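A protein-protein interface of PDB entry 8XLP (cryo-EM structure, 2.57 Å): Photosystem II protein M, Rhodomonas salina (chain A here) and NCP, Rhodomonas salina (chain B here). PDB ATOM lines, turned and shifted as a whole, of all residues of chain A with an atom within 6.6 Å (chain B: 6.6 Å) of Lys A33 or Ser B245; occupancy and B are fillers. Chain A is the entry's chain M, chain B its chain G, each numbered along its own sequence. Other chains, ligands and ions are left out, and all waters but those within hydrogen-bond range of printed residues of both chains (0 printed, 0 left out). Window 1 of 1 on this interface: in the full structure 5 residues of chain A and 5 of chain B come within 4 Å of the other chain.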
ATOM      1  N   PHE A  26      22.210 -16.221   4.413  1.00  0.00           N
ATOM      2  CA  PHE A  26      21.395 -15.169   5.015  1.00  0.00           C
ATOM      3  C   PHE A  26      20.377 -15.743   5.992  1.00  0.00           C
ATOM      4  O   PHE A  26      20.149 -15.170   7.065  1.00  0.00           O
ATOM      5  CB  PHE A  26      20.697 -14.361   3.921  1.00  0.00           C
ATOM      6  CG  PHE A  26      19.631 -13.434   4.435  1.00  0.00           C
ATOM      7  CD1 PHE A  26      19.968 -12.236   5.041  1.00  0.00           C
ATOM      8  CD2 PHE A  26      18.290 -13.757   4.300  1.00  0.00           C
ATOM      9  CE1 PHE A  26      18.989 -11.382   5.511  1.00  0.00           C
ATOM     10  CE2 PHE A  26      17.306 -12.904   4.765  1.00  0.00           C
ATOM     11  CZ  PHE A  26      17.656 -11.715   5.369  1.00  0.00           C
ATOM     12  N   GLN A  28      20.650 -18.560   7.657  1.00  0.00           N
ATOM     13  CA  GLN A  28      21.398 -18.997   8.832  1.00  0.00           C
ATOM     14  C   GLN A  28      21.737 -17.823   9.748  1.00  0.00           C
ATOM     15  O   GLN A  28      21.601 -17.920  10.977  1.00  0.00           O
ATOM     16  CB  GLN A  28      22.666 -19.730   8.386  1.00  0.00           C
ATOM     17  CG  GLN A  28      23.728 -19.907   9.460  1.00  0.00           C
ATOM     18  CD  GLN A  28      24.811 -18.850   9.392  1.00  0.00           C
ATOM     19  OE1 GLN A  28      24.901 -18.098   8.422  1.00  0.00           O
ATOM     20  NE2 GLN A  28      25.641 -18.787  10.427  1.00  0.00           N
ATOM     21  N   SER A  29      22.176 -16.702   9.166  1.00  0.00           N
ATOM     22  CA  SER A  29      22.497 -15.528   9.974  1.00  0.00           C
ATOM     23  C   SER A  29      21.262 -14.980  10.682  1.00  0.00           C
ATOM     24  O   SER A  29      21.318 -14.633  11.870  1.00  0.00           O
ATOM     25  CB  SER A  29      23.134 -14.449   9.100  1.00  0.00           C
ATOM     26  OG  SER A  29      23.467 -13.304   9.866  1.00  0.00           O
ATOM     27  N   GLU A  30      20.135 -14.898   9.969  1.00  0.00           N
ATOM     28  CA  GLU A  30      18.901 -14.425  10.589  1.00  0.00           C
ATOM     29  C   GLU A  30      18.424 -15.384  11.670  1.00  0.00           C
ATOM     30  O   GLU A  30      17.864 -14.957  12.686  1.00  0.00           O
ATOM     31  CB  GLU A  30      17.816 -14.233   9.528  1.00  0.00           C
ATOM     32  CG  GLU A  30      18.077 -13.094   8.554  1.00  0.00           C
ATOM     33  CD  GLU A  30      17.728 -11.728   9.120  1.00  0.00           C
ATOM     34  OE1 GLU A  30      18.374 -11.292  10.096  1.00  0.00           O
ATOM     35  OE2 GLU A  30      16.797 -11.087   8.586  1.00  0.00           O
ATOM     36  N   ALA A  31      18.630 -16.687  11.464  1.00  0.00           N
ATOM     37  CA  ALA A  31      18.274 -17.672  12.475  1.00  0.00           C
ATOM     38  C   ALA A  31      19.091 -17.480  13.743  1.00  0.00           C
ATOM     39  O   ALA A  31      18.550 -17.541  14.853  1.00  0.00           O
ATOM     40  CB  ALA A  31      18.477 -19.078  11.918  1.00  0.00           C
ATOM     41  N   ARG A  32      20.399 -17.248  13.598  1.00  0.00           N
ATOM     42  CA  ARG A  32      21.229 -16.977  14.769  1.00  0.00           C
ATOM     43  C   ARG A  32      20.792 -15.696  15.469  1.00  0.00           C
ATOM     44  O   ARG A  32      20.727 -15.645  16.705  1.00  0.00           O
ATOM     45  CB  ARG A  32      22.701 -16.893  14.371  1.00  0.00           C
ATOM     46  CG  ARG A  32      23.273 -18.188  13.834  1.00  0.00           C
ATOM     47  CD  ARG A  32      24.782 -18.113  13.693  1.00  0.00           C
ATOM     48  NE  ARG A  32      25.435 -17.930  14.982  1.00  0.00           N
ATOM     49  CZ  ARG A  32      25.884 -18.918  15.744  1.00  0.00           C
ATOM     50  NH1 ARG A  32      25.775 -20.183  15.370  1.00  0.00           N
ATOM     51  NH2 ARG A  32      26.457 -18.631  16.909  1.00  0.00           N
ATOM     52  N   LYS A  33      20.486 -14.651  14.693  1.00  0.00           N
ATOM     53  CA  LYS A  33      20.037 -13.392  15.282  1.00  0.00           C
ATOM     54  C   LYS A  33      18.736 -13.567  16.057  1.00  0.00           C
ATOM     55  O   LYS A  33      18.587 -13.033  17.163  1.00  0.00           O
ATOM     56  CB  LYS A  33      19.866 -12.335  14.192  1.00  0.00           C
ATOM     57  CG  LYS A  33      21.166 -11.783  13.636  1.00  0.00           C
ATOM     58  CD  LYS A  33      20.905 -10.892  12.432  1.00  0.00           C
ATOM     59  CE  LYS A  33      19.860  -9.830  12.743  1.00  0.00           C
ATOM     60  NZ  LYS A  33      19.527  -9.007  11.548  1.00  0.00           N
ATOM     61  N   ALA A  34      17.783 -14.311  15.492  1.00  0.00           N
ATOM     62  CA  ALA A  34      16.504 -14.518  16.163  1.00  0.00           C
ATOM     63  C   ALA A  34      16.656 -15.409  17.390  1.00  0.00           C
ATOM     64  O   ALA A  34      15.979 -15.200  18.403  1.00  0.00           O
ATOM     65  CB  ALA A  34      15.489 -15.112  15.189  1.00  0.00           C
ATOM     66  N   ALA A  35      17.528 -16.419  17.314  1.00  0.00           N
ATOM     67  CA  ALA A  35      17.743 -17.300  18.456  1.00  0.00           C
ATOM     68  C   ALA A  35      18.400 -16.560  19.614  1.00  0.00           C
ATOM     69  O   ALA A  35      18.006 -16.735  20.772  1.00  0.00           O
ATOM     70  CB  ALA A  35      18.588 -18.502  18.036  1.00  0.00           C
ATOM     71  N   GLU A  36      19.406 -15.733  19.321  1.00  0.00           N
ATOM     72  CA  GLU A  36      20.089 -15.000  20.384  1.00  0.00           C
ATOM     73  C   GLU A  36      19.194 -13.921  20.983  1.00  0.00           C
ATOM     74  O   GLU A  36      19.233 -13.677  22.195  1.00  0.00           O
ATOM     75  CB  GLU A  36      21.387 -14.404  19.849  1.00  0.00           C
ATOM     76  CG  GLU A  36      22.439 -15.455  19.554  1.00  0.00           C
ATOM     77  CD  GLU A  36      23.352 -15.065  18.416  1.00  0.00           C
ATOM     78  OE1 GLU A  36      23.069 -14.050  17.746  1.00  0.00           O
ATOM     79  OE2 GLU A  36      24.357 -15.770  18.192  1.00  0.00           O
ATOM     80  N   SER A  37      18.386 -13.266  20.156  1.00  0.00           N
ATOM     81  CA  SER A  37      17.470 -12.250  20.646  1.00  0.00           C
ATOM     82  C   SER A  37      16.235 -12.896  21.268  1.00  0.00           C
ATOM     83  O   SER A  37      15.958 -14.084  21.078  1.00  0.00           O
ATOM     84  CB  SER A  37      17.053 -11.308  19.516  1.00  0.00           C
ATOM     85  OG  SER A  37      16.368 -12.012  18.495  1.00  0.00           O
ATOM     86  N   GLY A  38      15.498 -12.095  22.034  1.00  0.00           N
ATOM     87  CA  GLY A  38      14.264 -12.554  22.640  1.00  0.00           C
ATOM     88  C   GLY A  38      13.194 -12.914  21.630  1.00  0.00           C
ATOM     89  O   GLY A  38      12.853 -12.105  20.761  1.00  0.00           O
ATOM     90  N   GLN A  39      12.652 -14.123  21.737  1.00  0.00           N
ATOM     91  CA  GLN A  39      11.601 -14.582  20.835  1.00  0.00           C
ATOM     92  C   GLN A  39      10.571 -15.426  21.577  1.00  0.00           C
ATOM     93  O   GLN A  39      10.855 -16.549  21.992  1.00  0.00           O
ATOM     94  CB  GLN A  39      12.197 -15.382  19.672  1.00  0.00           C
ATOM     95  CG  GLN A  39      12.737 -14.532  18.528  1.00  0.00           C
ATOM     96  CD  GLN A  39      11.636 -13.919  17.681  1.00  0.00           C
ATOM     97  OE1 GLN A  39      10.475 -14.323  17.762  1.00  0.00           O
ATOM     98  NE2 GLN A  39      11.997 -12.939  16.861  1.00  0.00           N
ATOM     99  N   GLY B 242      12.592  -0.075  17.019  1.00  0.00           N
ATOM    100  CA  GLY B 242      12.356  -0.758  15.762  1.00  0.00           C
ATOM    101  C   GLY B 242      13.269  -1.949  15.559  1.00  0.00           C
ATOM    102  O   GLY B 242      13.004  -3.038  16.076  1.00  0.00           O
ATOM    103  N   ASN B 243      14.349  -1.753  14.802  1.00  0.00           N
ATOM    104  CA  ASN B 243      15.301  -2.822  14.539  1.00  0.00           C
ATOM    105  C   ASN B 243      16.526  -2.620  15.418  1.00  0.00           C
ATOM    106  O   ASN B 243      17.334  -1.721  15.137  1.00  0.00           O
ATOM    107  CB  ASN B 243      15.696  -2.837  13.064  1.00  0.00           C
ATOM    108  CG  ASN B 243      16.451  -4.094  12.674  1.00  0.00           C
ATOM    109  OD1 ASN B 243      16.231  -5.164  13.238  1.00  0.00           O
ATOM    110  ND2 ASN B 243      17.346  -3.967  11.701  1.00  0.00           N
ATOM    111  N   PRO B 244      16.712  -3.414  16.476  1.00  0.00           N
ATOM    112  CA  PRO B 244      17.872  -3.203  17.354  1.00  0.00           C
ATOM    113  C   PRO B 244      19.155  -3.831  16.842  1.00  0.00           C
ATOM    114  O   PRO B 244      20.236  -3.448  17.311  1.00  0.00           O
ATOM    115  CB  PRO B 244      17.430  -3.856  18.670  1.00  0.00           C
ATOM    116  CG  PRO B 244      16.529  -4.964  18.228  1.00  0.00           C
ATOM    117  CD  PRO B 244      15.822  -4.476  16.981  1.00  0.00           C
ATOM    118  N   SER B 245      19.076  -4.774  15.908  1.00  0.00           N
ATOM    119  CA  SER B 245      20.244  -5.498  15.427  1.00  0.00           C
ATOM    120  C   SER B 245      20.908  -4.842  14.222  1.00  0.00           C
ATOM    121  O   SER B 245      21.906  -5.375  13.723  1.00  0.00           O
ATOM    122  CB  SER B 245      19.860  -6.938  15.076  1.00  0.00           C
ATOM    123  OG  SER B 245      18.842  -6.971  14.092  1.00  0.00           O
ATOM    124  N   PHE B 246      20.385  -3.717  13.740  1.00  0.00           N
ATOM    125  CA  PHE B 246      20.988  -3.049  12.594  1.00  0.00           C
ATOM    126  C   PHE B 246      22.350  -2.474  12.960  1.00  0.00           C
ATOM    127  O   PHE B 246      22.545  -1.936  14.053  1.00  0.00           O
ATOM    128  CB  PHE B 246      20.079  -1.936  12.074  1.00  0.00           C
ATOM    129  CG  PHE B 246      20.637  -1.210  10.880  1.00  0.00           C
ATOM    130  CD1 PHE B 246      20.461  -1.717   9.603  1.00  0.00           C
ATOM    131  CD2 PHE B 246      21.344  -0.026  11.034  1.00  0.00           C
ATOM    132  CE1 PHE B 246      20.976  -1.057   8.503  1.00  0.00           C
ATOM    133  CE2 PHE B 246      21.866   0.635   9.938  1.00  0.00           C
ATOM    134  CZ  PHE B 246      21.679   0.120   8.670  1.00  0.00           C
ATOM    135  N   GLY B 247      23.299  -2.598  12.034  1.00  0.00           N
ATOM    136  CA  GLY B 247      24.613  -2.019  12.221  1.00  0.00           C
ATOM    137  C   GLY B 247      25.499  -2.748  13.202  1.00  0.00           C
ATOM    138  O   GLY B 247      26.591  -2.261  13.508  1.00  0.00           O
ATOM    139  N   ARG B 248      25.066  -3.901  13.701  1.00  0.00           N
ATOM    140  CA  ARG B 248      25.816  -4.670  14.681  1.00  0.00           C
ATOM    141  C   ARG B 248      26.120  -6.051  14.120  1.00  0.00           C
ATOM    142  O   ARG B 248      25.270  -6.672  13.474  1.00  0.00           O
ATOM    143  CB  ARG B 248      25.039  -4.795  15.996  1.00  0.00           C
ATOM    144  CG  ARG B 248      24.806  -3.470  16.704  1.00  0.00           C
ATOM    145  CD  ARG B 248      23.997  -3.655  17.977  1.00  0.00           C
ATOM    146  NE  ARG B 248      23.942  -2.432  18.769  1.00  0.00           N
ATOM    147  CZ  ARG B 248      24.815  -2.115  19.715  1.00  0.00           C
ATOM    148  NH1 ARG B 248      25.825  -2.913  20.020  1.00  0.00           N
ATOM    149  NH2 ARG B 248      24.672  -0.967  20.372  1.00  0.00           N
ATOM    150  N   SER B 249      27.338  -6.523  14.367  1.00  0.00           N
ATOM    151  CA  SER B 249      27.734  -7.851  13.932  1.00  0.00           C
ATOM    152  C   SER B 249      26.986  -8.915  14.733  1.00  0.00           C
ATOM    153  O   SER B 249      26.336  -8.633  15.744  1.00  0.00           O
ATOM    154  CB  SER B 249      29.243  -8.035  14.077  1.00  0.00           C
ATOM    155  OG  SER B 249      29.640  -9.339  13.692  1.00  0.00           O
ATOM    156  N   LEU B 250      27.070 -10.158  14.252  1.00  0.00           N
ATOM    157  CA  LEU B 250      26.390 -11.257  14.930  1.00  0.00           C
ATOM    158  C   LEU B 250      26.941 -11.467  16.334  1.00  0.00           C
ATOM    159  O   LEU B 250      26.174 -11.662  17.284  1.00  0.00           O
ATOM    160  CB  LEU B 250      26.509 -12.538  14.103  1.00  0.00           C
ATOM    161  CG  LEU B 250      25.568 -13.693  14.462  1.00  0.00           C
ATOM    162  CD1 LEU B 250      25.153 -14.435  13.207  1.00  0.00           C
ATOM    163  CD2 LEU B 250      26.207 -14.656  15.454  1.00  0.00           C
ATOM    164  N   TYR B 253      25.895  -8.473  18.660  1.00  0.00           N
ATOM    165  CA  TYR B 253      24.493  -8.585  19.044  1.00  0.00           C
ATOM    166  C   TYR B 253      24.282  -9.736  20.019  1.00  0.00           C
ATOM    167  O   TYR B 253      23.507  -9.616  20.976  1.00  0.00           O
ATOM    168  CB  TYR B 253      23.624  -8.762  17.798  1.00  0.00           C
ATOM    169  CG  TYR B 253      22.138  -8.637  18.048  1.00  0.00           C
ATOM    170  CD1 TYR B 253      21.572  -7.412  18.378  1.00  0.00           C
ATOM    171  CD2 TYR B 253      21.300  -9.739  17.940  1.00  0.00           C
ATOM    172  CE1 TYR B 253      20.214  -7.290  18.604  1.00  0.00           C
ATOM    173  CE2 TYR B 253      19.939  -9.626  18.162  1.00  0.00           C
ATOM    174  CZ  TYR B 253      19.402  -8.400  18.493  1.00  0.00           C
ATOM    175  OH  TYR B 253      18.049  -8.281  18.716  1.00  0.00           O
ATOM    176  N   GLN B 256      25.600  -8.599  23.454  1.00  0.00           N
ATOM    177  CA  GLN B 256      24.733  -7.622  24.106  1.00  0.00           C
ATOM    178  C   GLN B 256      23.406  -8.244  24.534  1.00  0.00           C
ATOM    179  O   GLN B 256      22.818  -7.808  25.529  1.00  0.00           O
ATOM    180  CB  GLN B 256      24.505  -6.408  23.201  1.00  0.00           C
ATOM    181  CG  GLN B 256      23.443  -6.569  22.130  1.00  0.00           C
ATOM    182  CD  GLN B 256      22.949  -5.236  21.608  1.00  0.00           C
ATOM    183  OE1 GLN B 256      23.496  -4.185  21.944  1.00  0.00           O
ATOM    184  NE2 GLN B 256      21.904  -5.269  20.790  1.00  0.00           N
ATOM    185  N   THR B 257      22.916  -9.256  23.809  1.00  0.00           N
ATOM    186  CA  THR B 257      21.686  -9.922  24.223  1.00  0.00           C
ATOM    187  C   THR B 257      21.910 -10.883  25.384  1.00  0.00           C
ATOM    188  O   THR B 257      20.986 -11.116  26.173  1.00  0.00           O
ATOM    189  CB  THR B 257      21.059 -10.668  23.043  1.00  0.00           C
ATOM    190  OG1 THR B 257      22.063 -11.439  22.371  1.00  0.00           O
ATOM    191  CG2 THR B 257      20.429  -9.686  22.064  1.00  0.00           C
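The side-chain amino group (NZ) of Lys A33 lies close to the side-chain hydroxyl (OG) of Ser B245 (3.3 Å).
Of the 12 printed residues of chain B, 4 touch a printed residue of chain A. Printed residues of chain B that touch a printed residue of chain A: Ser B245, Leu B250, Tyr B253 and Thr B257. Hydrophobic or aromatic side chains of chain B within 4 Å of the printed part of chain A: Leu B250 and Tyr B253. Printed residues of chain A that touch a printed residue of chain B: Ser A29, Arg A32, Lys A33, Glu A36 and Ser A37. Among the printed residues, 7 pairs touch across the chains. Among the printed residues, no Asp or Glu carboxylate lies within 4 Å of a Lys or Arg side-chain nitrogen of the other chain.
The side-chain hydroxyl of Ser A37 sits at hydrogen-bond distance from the backbone carbonyl oxygen of Lys A33. O of Ala A34 sits at hydrogen-bond distance from OG of Ser A37, at 3.2 Å. OE1 of Glu A30 lies within salt-bridge range of NZ of Lys A33 (2.9 Å). The side-chain amide oxygen (OD1) of Asn B243 is in hydrogen-bond range of the side-chain hydroxyl (OG) of Ser B245. O of Tyr B253 lies within hydrogen-bond range of OG1 of Thr B257. The guanidinium group (NH2) of Arg A32 is in salt-bridge range of the side-chain carboxylate (OE2) of Glu A36 (3.8 Å).
Ser A29 touches Leu B250. Leu B250 touches Arg A32 (CD2 to NE, 3.4 Å). O of Lys A33 touches CE2 of Tyr B253, at 3.8 Å. OE2 of Glu A36 touches CD2 of Leu B250, 3.5 Å away. Thr B257 touches Glu A36 (OG1 to O, 3.6 Å). CB of Ser A37 touches OH of Tyr B253 (3.3 Å).
Of the printed residues of chain B, Arg A32 touches Leu B250 (3.4 Å). Lys A33 touches just these residues of chain B: Ser B245 (3.3 Å) and Tyr B253 (3.8 Å). Of the printed residues of chain B, Glu A36 touches Leu B250 (3.5 Å) and Thr B257 (3.6 Å). Ser B245 touches just one residue of chain A: Lys A33 (3.3 Å). Arg B248 touches none of the printed residues of chain A. Of the printed residues of chain A, Thr B257 touches Glu A36 (3.6 Å). The nearest printed residue of chain B that does not touch Arg A32 is Tyr B253 (6.1 Å).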
